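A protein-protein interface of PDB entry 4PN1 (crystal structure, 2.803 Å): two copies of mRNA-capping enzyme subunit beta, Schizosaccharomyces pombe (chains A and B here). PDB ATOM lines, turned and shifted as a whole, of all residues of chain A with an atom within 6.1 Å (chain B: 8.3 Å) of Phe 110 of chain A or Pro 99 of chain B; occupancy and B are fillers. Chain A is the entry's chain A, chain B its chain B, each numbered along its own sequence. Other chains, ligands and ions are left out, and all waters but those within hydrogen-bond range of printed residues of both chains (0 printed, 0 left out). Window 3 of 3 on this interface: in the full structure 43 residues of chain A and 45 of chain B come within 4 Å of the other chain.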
ATOM      1  N   PHE A  98     -29.915  32.879   4.607  1.00  0.00           N
ATOM      2  CA  PHE A  98     -30.650  32.119   5.614  1.00  0.00           C
ATOM      3  C   PHE A  98     -31.887  32.887   6.076  1.00  0.00           C
ATOM      4  O   PHE A  98     -31.798  34.067   6.412  1.00  0.00           O
ATOM      5  CB  PHE A  98     -29.733  31.826   6.804  1.00  0.00           C
ATOM      6  CG  PHE A  98     -29.969  30.492   7.448  1.00  0.00           C
ATOM      7  CD1 PHE A  98     -30.078  29.344   6.681  1.00  0.00           C
ATOM      8  CD2 PHE A  98     -30.052  30.380   8.827  1.00  0.00           C
ATOM      9  CE1 PHE A  98     -30.285  28.112   7.274  1.00  0.00           C
ATOM     10  CE2 PHE A  98     -30.258  29.152   9.427  1.00  0.00           C
ATOM     11  CZ  PHE A  98     -30.375  28.016   8.650  1.00  0.00           C
ATOM     12  N   THR A 104     -27.473  34.830  14.627  1.00  0.00           N
ATOM     13  CA  THR A 104     -27.795  33.466  15.024  1.00  0.00           C
ATOM     14  C   THR A 104     -26.613  32.510  14.872  1.00  0.00           C
ATOM     15  O   THR A 104     -25.912  32.517  13.859  1.00  0.00           O
ATOM     16  CB  THR A 104     -29.018  32.927  14.243  1.00  0.00           C
ATOM     17  OG1 THR A 104     -29.254  31.560  14.599  1.00  0.00           O
ATOM     18  CG2 THR A 104     -28.785  33.021  12.748  1.00  0.00           C
ATOM     19  N   ILE A 105     -26.395  31.697  15.898  1.00  0.00           N
ATOM     20  CA  ILE A 105     -25.364  30.671  15.859  1.00  0.00           C
ATOM     21  C   ILE A 105     -25.823  29.519  14.972  1.00  0.00           C
ATOM     22  O   ILE A 105     -26.972  29.089  15.052  1.00  0.00           O
ATOM     23  CB  ILE A 105     -25.072  30.126  17.272  1.00  0.00           C
ATOM     24  CG1 ILE A 105     -24.785  31.274  18.240  1.00  0.00           C
ATOM     25  CG2 ILE A 105     -23.910  29.146  17.243  1.00  0.00           C
ATOM     26  CD1 ILE A 105     -24.599  30.827  19.671  1.00  0.00           C
ATOM     27  N   LEU A 106     -24.931  29.028  14.120  1.00  0.00           N
ATOM     28  CA  LEU A 106     -25.242  27.875  13.283  1.00  0.00           C
ATOM     29  C   LEU A 106     -24.842  26.581  13.986  1.00  0.00           C
ATOM     30  O   LEU A 106     -23.779  26.502  14.600  1.00  0.00           O
ATOM     31  CB  LEU A 106     -24.530  27.980  11.933  1.00  0.00           C
ATOM     32  CG  LEU A 106     -24.903  29.167  11.045  1.00  0.00           C
ATOM     33  CD1 LEU A 106     -24.169  29.084   9.722  1.00  0.00           C
ATOM     34  CD2 LEU A 106     -26.407  29.226  10.823  1.00  0.00           C
ATOM     35  N   ASN A 107     -25.702  25.570  13.896  1.00  0.00           N
ATOM     36  CA  ASN A 107     -25.420  24.271  14.496  1.00  0.00           C
ATOM     37  C   ASN A 107     -24.344  23.533  13.704  1.00  0.00           C
ATOM     38  O   ASN A 107     -24.562  23.161  12.553  1.00  0.00           O
ATOM     39  CB  ASN A 107     -26.697  23.431  14.576  1.00  0.00           C
ATOM     40  CG  ASN A 107     -26.569  22.251  15.526  1.00  0.00           C
ATOM     41  OD1 ASN A 107     -25.482  21.713  15.730  1.00  0.00           O
ATOM     42  ND2 ASN A 107     -27.690  21.842  16.111  1.00  0.00           N
ATOM     43  N   PRO A 108     -23.176  23.318  14.327  1.00  0.00           N
ATOM     44  CA  PRO A 108     -22.033  22.693  13.653  1.00  0.00           C
ATOM     45  C   PRO A 108     -22.256  21.220  13.309  1.00  0.00           C
ATOM     46  O   PRO A 108     -21.485  20.659  12.530  1.00  0.00           O
ATOM     47  CB  PRO A 108     -20.905  22.834  14.682  1.00  0.00           C
ATOM     48  CG  PRO A 108     -21.599  22.930  15.993  1.00  0.00           C
ATOM     49  CD  PRO A 108     -22.867  23.678  15.721  1.00  0.00           C
ATOM     50  N   GLU A 109     -23.292  20.606  13.875  1.00  0.00           N
ATOM     51  CA  GLU A 109     -23.565  19.191  13.628  1.00  0.00           C
ATOM     52  C   GLU A 109     -24.257  18.960  12.285  1.00  0.00           C
ATOM     53  O   GLU A 109     -24.371  17.826  11.821  1.00  0.00           O
ATOM     54  CB  GLU A 109     -24.393  18.589  14.765  1.00  0.00           C
ATOM     55  CG  GLU A 109     -23.655  18.527  16.091  1.00  0.00           C
ATOM     56  CD  GLU A 109     -22.411  17.660  16.025  1.00  0.00           C
ATOM     57  OE1 GLU A 109     -22.509  16.514  15.537  1.00  0.00           O
ATOM     58  OE2 GLU A 109     -21.334  18.126  16.455  1.00  0.00           O
ATOM     59  N   PHE A 110     -24.717  20.041  11.666  1.00  0.00           N
ATOM     60  CA  PHE A 110     -25.328  19.963  10.346  1.00  0.00           C
ATOM     61  C   PHE A 110     -24.304  20.310   9.271  1.00  0.00           C
ATOM     62  O   PHE A 110     -23.355  21.055   9.522  1.00  0.00           O
ATOM     63  CB  PHE A 110     -26.523  20.912  10.249  1.00  0.00           C
ATOM     64  CG  PHE A 110     -27.739  20.448  11.003  1.00  0.00           C
ATOM     65  CD1 PHE A 110     -28.846  19.962  10.326  1.00  0.00           C
ATOM     66  CD2 PHE A 110     -27.779  20.504  12.388  1.00  0.00           C
ATOM     67  CE1 PHE A 110     -29.968  19.536  11.015  1.00  0.00           C
ATOM     68  CE2 PHE A 110     -28.898  20.076  13.084  1.00  0.00           C
ATOM     69  CZ  PHE A 110     -29.994  19.593  12.396  1.00  0.00           C
ATOM     70  N   ASN A 111     -24.498  19.762   8.076  1.00  0.00           N
ATOM     71  CA  ASN A 111     -23.654  20.081   6.930  1.00  0.00           C
ATOM     72  C   ASN A 111     -24.328  21.120   6.034  1.00  0.00           C
ATOM     73  O   ASN A 111     -25.150  20.780   5.180  1.00  0.00           O
ATOM     74  CB  ASN A 111     -23.329  18.807   6.147  1.00  0.00           C
ATOM     75  CG  ASN A 111     -22.421  19.062   4.959  1.00  0.00           C
ATOM     76  OD1 ASN A 111     -21.710  20.066   4.904  1.00  0.00           O
ATOM     77  ND2 ASN A 111     -22.441  18.146   3.998  1.00  0.00           N
ATOM     78  N   LEU A 112     -23.970  22.387   6.232  1.00  0.00           N
ATOM     79  CA  LEU A 112     -24.643  23.493   5.550  1.00  0.00           C
ATOM     80  C   LEU A 112     -24.014  23.913   4.215  1.00  0.00           C
ATOM     81  O   LEU A 112     -24.489  24.860   3.584  1.00  0.00           O
ATOM     82  CB  LEU A 112     -24.785  24.714   6.475  1.00  0.00           C
ATOM     83  CG  LEU A 112     -25.980  24.751   7.434  1.00  0.00           C
ATOM     84  CD1 LEU A 112     -25.674  23.967   8.667  1.00  0.00           C
ATOM     85  CD2 LEU A 112     -26.357  26.169   7.819  1.00  0.00           C
ATOM     86  N   PHE B  96     -40.653  21.902  14.400  1.00  0.00           N
ATOM     87  CA  PHE B  96     -39.747  22.386  13.371  1.00  0.00           C
ATOM     88  C   PHE B  96     -38.293  22.210  13.792  1.00  0.00           C
ATOM     89  O   PHE B  96     -37.955  22.355  14.967  1.00  0.00           O
ATOM     90  CB  PHE B  96     -40.043  23.859  13.085  1.00  0.00           C
ATOM     91  CG  PHE B  96     -39.289  24.418  11.916  1.00  0.00           C
ATOM     92  CD1 PHE B  96     -38.428  25.492  12.077  1.00  0.00           C
ATOM     93  CD2 PHE B  96     -39.445  23.874  10.652  1.00  0.00           C
ATOM     94  CE1 PHE B  96     -37.737  26.012  11.002  1.00  0.00           C
ATOM     95  CE2 PHE B  96     -38.756  24.387   9.572  1.00  0.00           C
ATOM     96  CZ  PHE B  96     -37.900  25.459   9.747  1.00  0.00           C
ATOM     97  N   GLU B  97     -37.438  21.879  12.831  1.00  0.00           N
ATOM     98  CA  GLU B  97     -36.008  21.787  13.091  1.00  0.00           C
ATOM     99  C   GLU B  97     -35.238  22.774  12.232  1.00  0.00           C
ATOM    100  O   GLU B  97     -35.598  23.032  11.085  1.00  0.00           O
ATOM    101  CB  GLU B  97     -35.494  20.370  12.862  1.00  0.00           C
ATOM    102  CG  GLU B  97     -36.038  19.360  13.849  1.00  0.00           C
ATOM    103  CD  GLU B  97     -35.143  18.145  13.990  1.00  0.00           C
ATOM    104  OE1 GLU B  97     -34.161  18.033  13.223  1.00  0.00           O
ATOM    105  OE2 GLU B  97     -35.420  17.307  14.873  1.00  0.00           O
ATOM    106  N   PHE B  98     -34.176  23.327  12.803  1.00  0.00           N
ATOM    107  CA  PHE B  98     -33.392  24.351  12.133  1.00  0.00           C
ATOM    108  C   PHE B  98     -31.975  24.332  12.690  1.00  0.00           C
ATOM    109  O   PHE B  98     -31.784  24.223  13.903  1.00  0.00           O
ATOM    110  CB  PHE B  98     -34.037  25.722  12.347  1.00  0.00           C
ATOM    111  CG  PHE B  98     -34.070  26.577  11.115  1.00  0.00           C
ATOM    112  CD1 PHE B  98     -34.437  26.041   9.893  1.00  0.00           C
ATOM    113  CD2 PHE B  98     -33.752  27.925  11.183  1.00  0.00           C
ATOM    114  CE1 PHE B  98     -34.473  26.828   8.756  1.00  0.00           C
ATOM    115  CE2 PHE B  98     -33.787  28.718  10.052  1.00  0.00           C
ATOM    116  CZ  PHE B  98     -34.149  28.167   8.837  1.00  0.00           C
ATOM    117  N   PRO B  99     -30.972  24.439  11.807  1.00  0.00           N
ATOM    118  CA  PRO B  99     -29.560  24.318  12.190  1.00  0.00           C
ATOM    119  C   PRO B  99     -29.056  25.517  12.989  1.00  0.00           C
ATOM    120  O   PRO B  99     -27.927  25.959  12.778  1.00  0.00           O
ATOM    121  CB  PRO B  99     -28.831  24.252  10.840  1.00  0.00           C
ATOM    122  CG  PRO B  99     -29.898  24.020   9.810  1.00  0.00           C
ATOM    123  CD  PRO B  99     -31.130  24.650  10.361  1.00  0.00           C
ATOM    124  N   VAL B 100     -29.881  26.026  13.895  1.00  0.00           N
ATOM    125  CA  VAL B 100     -29.512  27.168  14.722  1.00  0.00           C
ATOM    126  C   VAL B 100     -29.477  26.777  16.199  1.00  0.00           C
ATOM    127  O   VAL B 100     -30.146  25.832  16.616  1.00  0.00           O
ATOM    128  CB  VAL B 100     -30.480  28.344  14.513  1.00  0.00           C
ATOM    129  CG1 VAL B 100     -30.475  28.778  13.053  1.00  0.00           C
ATOM    130  CG2 VAL B 100     -31.879  27.958  14.949  1.00  0.00           C
ATOM    131  N   MET B 101     -28.695  27.507  16.988  1.00  0.00           N
ATOM    132  CA  MET B 101     -28.483  27.136  18.382  1.00  0.00           C
ATOM    133  C   MET B 101     -28.940  28.201  19.375  1.00  0.00           C
ATOM    134  O   MET B 101     -28.525  28.193  20.533  1.00  0.00           O
ATOM    135  CB  MET B 101     -27.010  26.804  18.627  1.00  0.00           C
ATOM    136  CG  MET B 101     -26.491  25.634  17.816  1.00  0.00           C
ATOM    137  SD  MET B 101     -24.864  25.109  18.381  1.00  0.00           S
ATOM    138  CE  MET B 101     -25.223  24.723  20.090  1.00  0.00           C
ATOM    139  N   ASN B 102     -29.794  29.114  18.927  1.00  0.00           N
ATOM    140  CA  ASN B 102     -30.311  30.155  19.807  1.00  0.00           C
ATOM    141  C   ASN B 102     -31.640  30.715  19.325  1.00  0.00           C
ATOM    142  O   ASN B 102     -32.057  30.461  18.195  1.00  0.00           O
ATOM    143  CB  ASN B 102     -29.294  31.289  19.958  1.00  0.00           C
ATOM    144  CG  ASN B 102     -28.962  31.956  18.638  1.00  0.00           C
ATOM    145  OD1 ASN B 102     -28.004  31.581  17.965  1.00  0.00           O
ATOM    146  ND2 ASN B 102     -29.756  32.953  18.261  1.00  0.00           N
ATOM    147  N   THR B 104     -34.085  32.599  17.541  1.00  0.00           N
ATOM    148  CA  THR B 104     -33.964  33.295  16.265  1.00  0.00           C
ATOM    149  C   THR B 104     -35.317  33.687  15.673  1.00  0.00           C
ATOM    150  O   THR B 104     -36.269  32.909  15.704  1.00  0.00           O
ATOM    151  CB  THR B 104     -33.180  32.455  15.239  1.00  0.00           C
ATOM    152  OG1 THR B 104     -33.340  33.024  13.936  1.00  0.00           O
ATOM    153  CG2 THR B 104     -33.691  31.029  15.221  1.00  0.00           C
ATOM    154  N   TYR B 195     -38.078  30.834  16.746  1.00  0.00           N
ATOM    155  CA  TYR B 195     -37.679  29.444  16.933  1.00  0.00           C
ATOM    156  C   TYR B 195     -36.638  29.343  18.048  1.00  0.00           C
ATOM    157  O   TYR B 195     -35.602  30.008  18.002  1.00  0.00           O
ATOM    158  CB  TYR B 195     -37.132  28.873  15.621  1.00  0.00           C
ATOM    159  CG  TYR B 195     -36.595  27.467  15.736  1.00  0.00           C
ATOM    160  CD1 TYR B 195     -37.453  26.379  15.801  1.00  0.00           C
ATOM    161  CD2 TYR B 195     -35.229  27.226  15.776  1.00  0.00           C
ATOM    162  CE1 TYR B 195     -36.965  25.093  15.908  1.00  0.00           C
ATOM    163  CE2 TYR B 195     -34.731  25.942  15.883  1.00  0.00           C
ATOM    164  CZ  TYR B 195     -35.603  24.879  15.947  1.00  0.00           C
ATOM    165  OH  TYR B 195     -35.113  23.598  16.054  1.00  0.00           O
ATOM    166  N   PRO B 197     -34.572  26.561  19.946  1.00  0.00           N
ATOM    167  CA  PRO B 197     -34.117  25.167  20.044  1.00  0.00           C
ATOM    168  C   PRO B 197     -33.665  24.717  21.438  1.00  0.00           C
ATOM    169  O   PRO B 197     -33.558  23.515  21.674  1.00  0.00           O
ATOM    170  CB  PRO B 197     -32.943  25.112  19.057  1.00  0.00           C
ATOM    171  CG  PRO B 197     -32.487  26.525  18.923  1.00  0.00           C
ATOM    172  CD  PRO B 197     -33.725  27.356  19.041  1.00  0.00           C
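The side-chain amide oxygen (OD1) of Asn 107 of chain A is in hydrogen-bond range of the backbone NH (N) of Glu 109 of chain A (3.1 Å). The backbone NH (N) of Phe 98 of chain B lies within hydrogen-bond range of the side-chain hydroxyl (OH) of Tyr 195 of chain B.
N of Ile 105 of chain A is in hydrogen-bond range of OD1 of Asn 102 of chain B, at 2.6 Å. The backbone NH of Met 101 of chain B lies within hydrogen-bond range of the backbone carbonyl oxygen of Ile 105 of chain A, 3.0 Å away. The backbone NH of Asn 107 of chain A lies within hydrogen-bond range of the backbone carbonyl oxygen of Pro 99 of chain B, 2.5 Å away.
Of the printed residues of chain B, Phe 98 of chain A touches Phe 98 (3.6 Å), Pro 99 (3.9 Å) and Val 100 (3.7 Å). Printed residues of chain B within 4 Å of Thr 104 of chain A: Val 100 (3.4 Å) and Asn 102 (3.5 Å). Of the printed residues of chain B, Leu 106 of chain A touches Pro 99. Of chain B, only Pro 99 (3.96 Å) comes within 4 Å of Phe 110 of chain A. Of the printed residues of chain A, Phe 98 of chain B touches Phe 98. Of the printed residues of chain A, Pro 99 of chain B touches Phe 98 (3.9 Å), Ile 105 (3.98 Å), Leu 106 (3.3 Å), Asn 107 (2.5 Å), Phe 110 (3.96 Å) and Leu 112 (3.8 Å). Of the printed residues of chain A, Asn 102 of chain B touches Thr 104 and Ile 105. The nearest printed residue of chain A that does not touch Pro 99 of chain B is Pro 108 of chain A (5.7 Å).
Phe 98 of chain B touches Phe 98 of chain A. CZ of Phe 98 of chain A touches CD of Pro 99 of chain B, 3.9 Å away. Val 100 of chain B touches Thr 104 of chain A. Pro 99 of chain B touches Ile 105 of chain A. Ile 105 of chain A touches Val 100 of chain B (O to CA, 3.2 Å). Leu 106 of chain A touches Pro 99 of chain B (CA to O, 3.3 Å). Asn 107 of chain A touches Met 101 of chain B. Pro 108 of chain A touches Met 101 of chain B. Phe 110 of chain A touches Pro 99 of chain B. Pro 99 of chain B touches Leu 112 of chain A.
Phe 98 of chain A touches its own counterpart, Phe 98 of chain B.
Of the 10 printed residues of chain B, 5 touch a printed residue of chain A. Hydrophobic or aromatic side chains of chain B that line the printed part of chain A: Phe 98, Pro 99, Val 100 and Met 101. Along chain B the printed residues that touch a printed residue of chain A span positions 98 to 102. Hydrophobic or aromatic side chains of chain A that line the printed part of chain B: Phe 98, Ile 105, Pro 108, Phe 110 and Leu 112. Among the printed residues, 15 pairs touch across the chains. Among the printed residues, no Asp or Glu carboxylate lies within 4 Å of a Lys or Arg side-chain nitrogen of the other chain.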
